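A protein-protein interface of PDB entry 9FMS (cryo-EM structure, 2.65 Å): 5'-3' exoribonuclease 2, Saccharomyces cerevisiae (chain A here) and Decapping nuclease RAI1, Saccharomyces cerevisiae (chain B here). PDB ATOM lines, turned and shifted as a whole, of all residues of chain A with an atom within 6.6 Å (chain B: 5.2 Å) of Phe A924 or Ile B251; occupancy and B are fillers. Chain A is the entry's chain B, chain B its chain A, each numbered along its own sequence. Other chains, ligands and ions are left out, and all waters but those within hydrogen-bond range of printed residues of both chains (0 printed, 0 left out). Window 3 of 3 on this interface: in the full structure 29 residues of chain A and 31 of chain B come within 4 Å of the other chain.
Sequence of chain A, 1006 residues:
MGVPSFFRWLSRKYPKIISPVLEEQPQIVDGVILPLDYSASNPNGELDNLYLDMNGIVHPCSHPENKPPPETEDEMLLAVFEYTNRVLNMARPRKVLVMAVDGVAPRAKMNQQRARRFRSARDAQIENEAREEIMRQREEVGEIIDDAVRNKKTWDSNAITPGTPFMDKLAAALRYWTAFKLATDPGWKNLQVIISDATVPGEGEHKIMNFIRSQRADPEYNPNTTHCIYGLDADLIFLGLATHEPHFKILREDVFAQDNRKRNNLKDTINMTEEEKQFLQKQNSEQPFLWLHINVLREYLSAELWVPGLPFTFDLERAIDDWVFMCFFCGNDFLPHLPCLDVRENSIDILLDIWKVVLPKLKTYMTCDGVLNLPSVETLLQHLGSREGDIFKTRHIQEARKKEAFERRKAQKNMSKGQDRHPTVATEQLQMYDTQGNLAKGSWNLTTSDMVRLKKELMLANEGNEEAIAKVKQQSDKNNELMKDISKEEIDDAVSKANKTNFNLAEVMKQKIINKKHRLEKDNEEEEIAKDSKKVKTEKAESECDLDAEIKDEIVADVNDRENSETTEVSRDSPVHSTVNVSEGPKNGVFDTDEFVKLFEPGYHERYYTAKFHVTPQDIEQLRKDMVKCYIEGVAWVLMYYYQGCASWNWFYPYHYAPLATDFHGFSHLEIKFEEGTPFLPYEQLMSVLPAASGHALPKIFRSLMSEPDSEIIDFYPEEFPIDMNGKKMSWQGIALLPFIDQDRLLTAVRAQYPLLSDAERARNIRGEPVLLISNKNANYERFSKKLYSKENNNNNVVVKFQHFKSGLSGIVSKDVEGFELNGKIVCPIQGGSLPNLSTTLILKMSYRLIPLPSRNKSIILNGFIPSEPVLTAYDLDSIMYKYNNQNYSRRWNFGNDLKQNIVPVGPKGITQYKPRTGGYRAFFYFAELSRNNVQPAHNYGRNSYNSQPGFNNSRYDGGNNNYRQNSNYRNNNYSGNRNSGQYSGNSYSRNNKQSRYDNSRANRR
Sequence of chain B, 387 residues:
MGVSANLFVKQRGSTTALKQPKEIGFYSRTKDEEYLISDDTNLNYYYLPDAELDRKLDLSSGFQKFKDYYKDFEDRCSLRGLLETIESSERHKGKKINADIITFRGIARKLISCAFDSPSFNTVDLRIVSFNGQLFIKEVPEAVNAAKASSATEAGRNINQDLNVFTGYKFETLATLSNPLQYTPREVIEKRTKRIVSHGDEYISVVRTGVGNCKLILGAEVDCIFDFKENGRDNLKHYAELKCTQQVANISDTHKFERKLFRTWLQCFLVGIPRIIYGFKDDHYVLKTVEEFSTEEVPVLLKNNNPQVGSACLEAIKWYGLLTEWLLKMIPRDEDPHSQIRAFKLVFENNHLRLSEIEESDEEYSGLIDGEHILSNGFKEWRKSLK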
ATOM      1  N   ARG A 917      36.393   4.185   1.301  1.00  0.00           N
ATOM      2  CA  ARG A 917      35.604   4.475   2.507  1.00  0.00           C
ATOM      3  C   ARG A 917      34.141   4.553   2.117  1.00  0.00           C
ATOM      4  O   ARG A 917      33.855   4.978   1.011  1.00  0.00           O
ATOM      5  CB  ARG A 917      36.030   5.825   3.073  1.00  0.00           C
ATOM      6  CG  ARG A 917      37.448   5.893   3.627  1.00  0.00           C
ATOM      7  CD  ARG A 917      37.863   7.357   3.738  1.00  0.00           C
ATOM      8  NE  ARG A 917      39.294   7.501   4.026  1.00  0.00           N
ATOM      9  CZ  ARG A 917      39.825   7.499   5.218  1.00  0.00           C
ATOM     10  NH1 ARG A 917      41.074   7.778   5.399  1.00  0.00           N
ATOM     11  NH2 ARG A 917      39.129   7.250   6.277  1.00  0.00           N
ATOM     12  N   THR A 918      33.199   4.154   2.957  1.00  0.00           N
ATOM     13  CA  THR A 918      31.784   4.182   2.561  1.00  0.00           C
ATOM     14  C   THR A 918      31.314   5.603   2.329  1.00  0.00           C
ATOM     15  O   THR A 918      31.699   6.505   3.061  1.00  0.00           O
ATOM     16  CB  THR A 918      30.866   3.499   3.566  1.00  0.00           C
ATOM     17  OG1 THR A 918      31.070   4.027   4.844  1.00  0.00           O
ATOM     18  CG2 THR A 918      31.104   2.001   3.647  1.00  0.00           C
ATOM     19  N   GLY A 919      30.467   5.806   1.328  1.00  0.00           N
ATOM     20  CA  GLY A 919      30.091   7.139   0.873  1.00  0.00           C
ATOM     21  C   GLY A 919      31.031   7.676  -0.193  1.00  0.00           C
ATOM     22  O   GLY A 919      31.546   8.776  -0.073  1.00  0.00           O
ATOM     23  N   GLY A 920      31.313   6.893  -1.218  1.00  0.00           N
ATOM     24  CA  GLY A 920      32.157   7.293  -2.334  1.00  0.00           C
ATOM     25  C   GLY A 920      31.843   6.423  -3.531  1.00  0.00           C
ATOM     26  O   GLY A 920      31.499   5.261  -3.353  1.00  0.00           O
ATOM     27  N   TYR A 921      31.870   6.963  -4.743  1.00  0.00           N
ATOM     28  CA  TYR A 921      31.401   6.229  -5.913  1.00  0.00           C
ATOM     29  C   TYR A 921      32.214   4.967  -6.178  1.00  0.00           C
ATOM     30  O   TYR A 921      31.657   3.878  -6.286  1.00  0.00           O
ATOM     31  CB  TYR A 921      31.428   7.132  -7.139  1.00  0.00           C
ATOM     32  CG  TYR A 921      31.053   6.409  -8.413  1.00  0.00           C
ATOM     33  CD1 TYR A 921      29.700   6.242  -8.745  1.00  0.00           C
ATOM     34  CD2 TYR A 921      32.050   5.906  -9.268  1.00  0.00           C
ATOM     35  CE1 TYR A 921      29.345   5.627  -9.954  1.00  0.00           C
ATOM     36  CE2 TYR A 921      31.695   5.277 -10.471  1.00  0.00           C
ATOM     37  CZ  TYR A 921      30.341   5.150 -10.825  1.00  0.00           C
ATOM     38  OH  TYR A 921      29.997   4.560 -11.994  1.00  0.00           O
ATOM     39  N   ARG A 922      33.536   5.080  -6.260  1.00  0.00           N
ATOM     40  CA  ARG A 922      34.411   3.955  -6.545  1.00  0.00           C
ATOM     41  C   ARG A 922      34.455   3.008  -5.362  1.00  0.00           C
ATOM     42  O   ARG A 922      34.460   1.800  -5.555  1.00  0.00           O
ATOM     43  CB  ARG A 922      35.753   4.548  -6.935  1.00  0.00           C
ATOM     44  CG  ARG A 922      36.815   3.509  -7.241  1.00  0.00           C
ATOM     45  CD  ARG A 922      37.961   4.197  -7.989  1.00  0.00           C
ATOM     46  NE  ARG A 922      37.706   4.160  -9.428  1.00  0.00           N
ATOM     47  CZ  ARG A 922      38.319   4.844 -10.359  1.00  0.00           C
ATOM     48  NH1 ARG A 922      38.149   4.519 -11.592  1.00  0.00           N
ATOM     49  NH2 ARG A 922      39.113   5.838 -10.137  1.00  0.00           N
ATOM     50  N   ALA A 923      34.388   3.518  -4.144  1.00  0.00           N
ATOM     51  CA  ALA A 923      34.248   2.699  -2.954  1.00  0.00           C
ATOM     52  C   ALA A 923      32.947   1.897  -2.885  1.00  0.00           C
ATOM     53  O   ALA A 923      32.958   0.803  -2.332  1.00  0.00           O
ATOM     54  CB  ALA A 923      34.359   3.604  -1.740  1.00  0.00           C
ATOM     55  N   PHE A 924      31.833   2.365  -3.445  1.00  0.00           N
ATOM     56  CA  PHE A 924      30.572   1.630  -3.411  1.00  0.00           C
ATOM     57  C   PHE A 924      30.671   0.275  -4.107  1.00  0.00           C
ATOM     58  O   PHE A 924      30.273  -0.739  -3.546  1.00  0.00           O
ATOM     59  CB  PHE A 924      29.476   2.482  -4.041  1.00  0.00           C
ATOM     60  CG  PHE A 924      28.130   1.802  -4.136  1.00  0.00           C
ATOM     61  CD1 PHE A 924      27.794   1.057  -5.273  1.00  0.00           C
ATOM     62  CD2 PHE A 924      27.208   1.925  -3.091  1.00  0.00           C
ATOM     63  CE1 PHE A 924      26.554   0.418  -5.353  1.00  0.00           C
ATOM     64  CE2 PHE A 924      25.966   1.291  -3.174  1.00  0.00           C
ATOM     65  CZ  PHE A 924      25.641   0.530  -4.302  1.00  0.00           C
ATOM     66  N   PHE A 925      31.260   0.232  -5.304  1.00  0.00           N
ATOM     67  CA  PHE A 925      31.475  -1.019  -6.027  1.00  0.00           C
ATOM     68  C   PHE A 925      32.534  -1.896  -5.369  1.00  0.00           C
ATOM     69  O   PHE A 925      32.370  -3.111  -5.344  1.00  0.00           O
ATOM     70  CB  PHE A 925      31.837  -0.726  -7.478  1.00  0.00           C
ATOM     71  CG  PHE A 925      30.736   0.017  -8.193  1.00  0.00           C
ATOM     72  CD1 PHE A 925      29.574  -0.666  -8.587  1.00  0.00           C
ATOM     73  CD2 PHE A 925      30.836   1.399  -8.393  1.00  0.00           C
ATOM     74  CE1 PHE A 925      28.517   0.035  -9.184  1.00  0.00           C
ATOM     75  CE2 PHE A 925      29.775   2.098  -8.980  1.00  0.00           C
ATOM     76  CZ  PHE A 925      28.620   1.421  -9.384  1.00  0.00           C
ATOM     77  N   TYR A 926      33.575  -1.302  -4.779  1.00  0.00           N
ATOM     78  CA  TYR A 926      34.582  -2.051  -4.032  1.00  0.00           C
ATOM     79  C   TYR A 926      33.958  -2.832  -2.874  1.00  0.00           C
ATOM     80  O   TYR A 926      34.067  -4.049  -2.834  1.00  0.00           O
ATOM     81  CB  TYR A 926      35.672  -1.089  -3.557  1.00  0.00           C
ATOM     82  CG  TYR A 926      36.713  -1.718  -2.664  1.00  0.00           C
ATOM     83  CD1 TYR A 926      37.819  -2.368  -3.236  1.00  0.00           C
ATOM     84  CD2 TYR A 926      36.586  -1.642  -1.268  1.00  0.00           C
ATOM     85  CE1 TYR A 926      38.795  -2.947  -2.413  1.00  0.00           C
ATOM     86  CE2 TYR A 926      37.561  -2.220  -0.442  1.00  0.00           C
ATOM     87  CZ  TYR A 926      38.667  -2.872  -1.014  1.00  0.00           C
ATOM     88  OH  TYR A 926      39.611  -3.424  -0.218  1.00  0.00           O
ATOM     89  N   PHE A 927      33.236  -2.176  -1.965  1.00  0.00           N
ATOM     90  CA  PHE A 927      32.601  -2.870  -0.843  1.00  0.00           C
ATOM     91  C   PHE A 927      31.477  -3.817  -1.277  1.00  0.00           C
ATOM     92  O   PHE A 927      31.289  -4.852  -0.641  1.00  0.00           O
ATOM     93  CB  PHE A 927      32.097  -1.862   0.194  1.00  0.00           C
ATOM     94  CG  PHE A 927      33.212  -1.146   0.921  1.00  0.00           C
ATOM     95  CD1 PHE A 927      34.115  -1.882   1.707  1.00  0.00           C
ATOM     96  CD2 PHE A 927      33.373   0.241   0.789  1.00  0.00           C
ATOM     97  CE1 PHE A 927      35.186  -1.236   2.338  1.00  0.00           C
ATOM     98  CE2 PHE A 927      34.451   0.882   1.413  1.00  0.00           C
ATOM     99  CZ  PHE A 927      35.359   0.146   2.188  1.00  0.00           C
ATOM    100  N   ALA A 928      30.759  -3.531  -2.364  1.00  0.00           N
ATOM    101  CA  ALA A 928      29.782  -4.465  -2.910  1.00  0.00           C
ATOM    102  C   ALA A 928      30.453  -5.756  -3.406  1.00  0.00           C
ATOM    103  O   ALA A 928      30.050  -6.845  -2.997  1.00  0.00           O
ATOM    104  CB  ALA A 928      28.980  -3.770  -4.010  1.00  0.00           C
ATOM    105  N   GLU A 929      31.512  -5.664  -4.210  1.00  0.00           N
ATOM    106  CA  GLU A 929      32.261  -6.828  -4.704  1.00  0.00           C
ATOM    107  C   GLU A 929      32.954  -7.608  -3.573  1.00  0.00           C
ATOM    108  O   GLU A 929      33.030  -8.835  -3.614  1.00  0.00           O
ATOM    109  CB  GLU A 929      33.277  -6.352  -5.752  1.00  0.00           C
ATOM    110  CG  GLU A 929      34.085  -7.508  -6.358  1.00  0.00           C
ATOM    111  CD  GLU A 929      34.962  -7.094  -7.553  1.00  0.00           C
ATOM    112  OE1 GLU A 929      35.471  -5.949  -7.587  1.00  0.00           O
ATOM    113  OE2 GLU A 929      35.167  -7.928  -8.466  1.00  0.00           O
ATOM    114  N   VAL B 248      27.101   8.923  -1.667  1.00  0.00           N
ATOM    115  CA  VAL B 248      26.728   7.754  -2.493  1.00  0.00           C
ATOM    116  C   VAL B 248      26.513   6.542  -1.594  1.00  0.00           C
ATOM    117  O   VAL B 248      27.475   5.992  -1.070  1.00  0.00           O
ATOM    118  CB  VAL B 248      27.755   7.447  -3.604  1.00  0.00           C
ATOM    119  CG1 VAL B 248      27.375   6.198  -4.400  1.00  0.00           C
ATOM    120  CG2 VAL B 248      27.874   8.585  -4.617  1.00  0.00           C
ATOM    121  N   ALA B 249      25.264   6.123  -1.398  1.00  0.00           N
ATOM    122  CA  ALA B 249      24.914   5.094  -0.417  1.00  0.00           C
ATOM    123  C   ALA B 249      23.940   4.021  -0.933  1.00  0.00           C
ATOM    124  O   ALA B 249      23.583   3.104  -0.197  1.00  0.00           O
ATOM    125  CB  ALA B 249      24.353   5.809   0.812  1.00  0.00           C
ATOM    126  N   ASN B 250      23.493   4.119  -2.180  1.00  0.00           N
ATOM    127  CA  ASN B 250      22.454   3.282  -2.768  1.00  0.00           C
ATOM    128  C   ASN B 250      22.660   3.199  -4.283  1.00  0.00           C
ATOM    129  O   ASN B 250      23.304   4.072  -4.861  1.00  0.00           O
ATOM    130  CB  ASN B 250      21.098   3.916  -2.406  1.00  0.00           C
ATOM    131  CG  ASN B 250      19.912   3.047  -2.760  1.00  0.00           C
ATOM    132  OD1 ASN B 250      20.024   1.848  -2.967  1.00  0.00           O
ATOM    133  ND2 ASN B 250      18.741   3.623  -2.860  1.00  0.00           N
ATOM    134  N   ILE B 251      22.087   2.208  -4.959  1.00  0.00           N
ATOM    135  CA  ILE B 251      22.297   2.020  -6.401  1.00  0.00           C
ATOM    136  C   ILE B 251      21.886   3.269  -7.188  1.00  0.00           C
ATOM    137  O   ILE B 251      22.662   3.753  -8.006  1.00  0.00           O
ATOM    138  CB  ILE B 251      21.593   0.747  -6.913  1.00  0.00           C
ATOM    139  CG1 ILE B 251      22.165  -0.501  -6.204  1.00  0.00           C
ATOM    140  CG2 ILE B 251      21.774   0.615  -8.432  1.00  0.00           C
ATOM    141  CD1 ILE B 251      21.478  -1.819  -6.566  1.00  0.00           C
ATOM    142  N   SER B 252      20.735   3.876  -6.910  1.00  0.00           N
ATOM    143  CA  SER B 252      20.307   5.081  -7.635  1.00  0.00           C
ATOM    144  C   SER B 252      21.180   6.313  -7.362  1.00  0.00           C
ATOM    145  O   SER B 252      21.257   7.210  -8.199  1.00  0.00           O
ATOM    146  CB  SER B 252      18.842   5.374  -7.330  1.00  0.00           C
ATOM    147  OG  SER B 252      18.667   5.606  -5.952  1.00  0.00           O
ATOM    148  N   ASP B 253      21.929   6.364  -6.260  1.00  0.00           N
ATOM    149  CA  ASP B 253      22.934   7.410  -6.071  1.00  0.00           C
ATOM    150  C   ASP B 253      24.097   7.273  -7.049  1.00  0.00           C
ATOM    151  O   ASP B 253      24.646   8.282  -7.484  1.00  0.00           O
ATOM    152  CB  ASP B 253      23.488   7.427  -4.646  1.00  0.00           C
ATOM    153  CG  ASP B 253      22.461   7.691  -3.546  1.00  0.00           C
ATOM    154  OD1 ASP B 253      21.403   8.306  -3.817  1.00  0.00           O
ATOM    155  OD2 ASP B 253      22.767   7.318  -2.394  1.00  0.00           O
ATOM    156  N   THR B 254      24.456   6.055  -7.455  1.00  0.00           N
ATOM    157  CA  THR B 254      25.520   5.861  -8.441  1.00  0.00           C
ATOM    158  C   THR B 254      25.137   6.473  -9.784  1.00  0.00           C
ATOM    159  O   THR B 254      25.970   7.115 -10.414  1.00  0.00           O
ATOM    160  CB  THR B 254      25.913   4.391  -8.610  1.00  0.00           C
ATOM    161  OG1 THR B 254      24.937   3.660  -9.294  1.00  0.00           O
ATOM    162  CG2 THR B 254      26.175   3.681  -7.288  1.00  0.00           C
ATOM    163  N   HIS B 255      23.868   6.394 -10.187  1.00  0.00           N
ATOM    164  CA  HIS B 255      23.395   7.005 -11.428  1.00  0.00           C
ATOM    165  C   HIS B 255      23.297   8.527 -11.350  1.00  0.00           C
ATOM    166  O   HIS B 255      23.670   9.217 -12.296  1.00  0.00           O
ATOM    167  CB  HIS B 255      22.064   6.385 -11.847  1.00  0.00           C
ATOM    168  CG  HIS B 255      22.148   4.893 -12.022  1.00  0.00           C
ATOM    169  ND1 HIS B 255      23.223   4.195 -12.521  1.00  0.00           N
ATOM    170  CD2 HIS B 255      21.194   3.979 -11.680  1.00  0.00           C
ATOM    171  CE1 HIS B 255      22.926   2.886 -12.478  1.00  0.00           C
ATOM    172  NE2 HIS B 255      21.689   2.705 -11.982  1.00  0.00           N
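Of the printed residues of chain B, Phe A925 touches Thr B254.
Of the printed residues of chain A, Val B248 touches Gly A919 (3.5 Å) and Gly A920 (3.9 Å).
The nearest printed residue of chain B that does not touch Gly A920 is Ala B249 (6.1 Å).
N of Asn B250 is in hydrogen-bond range of OD2 of Asp B253 (3.3 Å).
The side-chain hydroxyl (OG1) of Thr B254 sits at hydrogen-bond distance from the backbone carbonyl oxygen (O) of Ile B251 (2.6 Å).
Gly A919 touches Val B248.
Val B248 touches Gly A920.
Thr B254 touches Tyr A921 (O to CE1, 3.7 Å).
Phe A924 touches Asn B250.
Phe A924 touches Ile B251.
CG2 of Thr B254 touches CD1 of Phe A924 (3.7 Å).
Phe A925 touches Thr B254.
Of the 13 printed residues of chain A, 5 touch a printed residue of chain B.
Hydrophobic or aromatic side chains of chain A that line the printed part of chain B: Tyr A921, Phe A924 and Phe A925.
Of the 8 printed residues of chain B, 4 touch a printed residue of chain A.
Printed residues of chain B that touch a printed residue of chain A: Val B248, Asn B250, Ile B251 and Thr B254.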
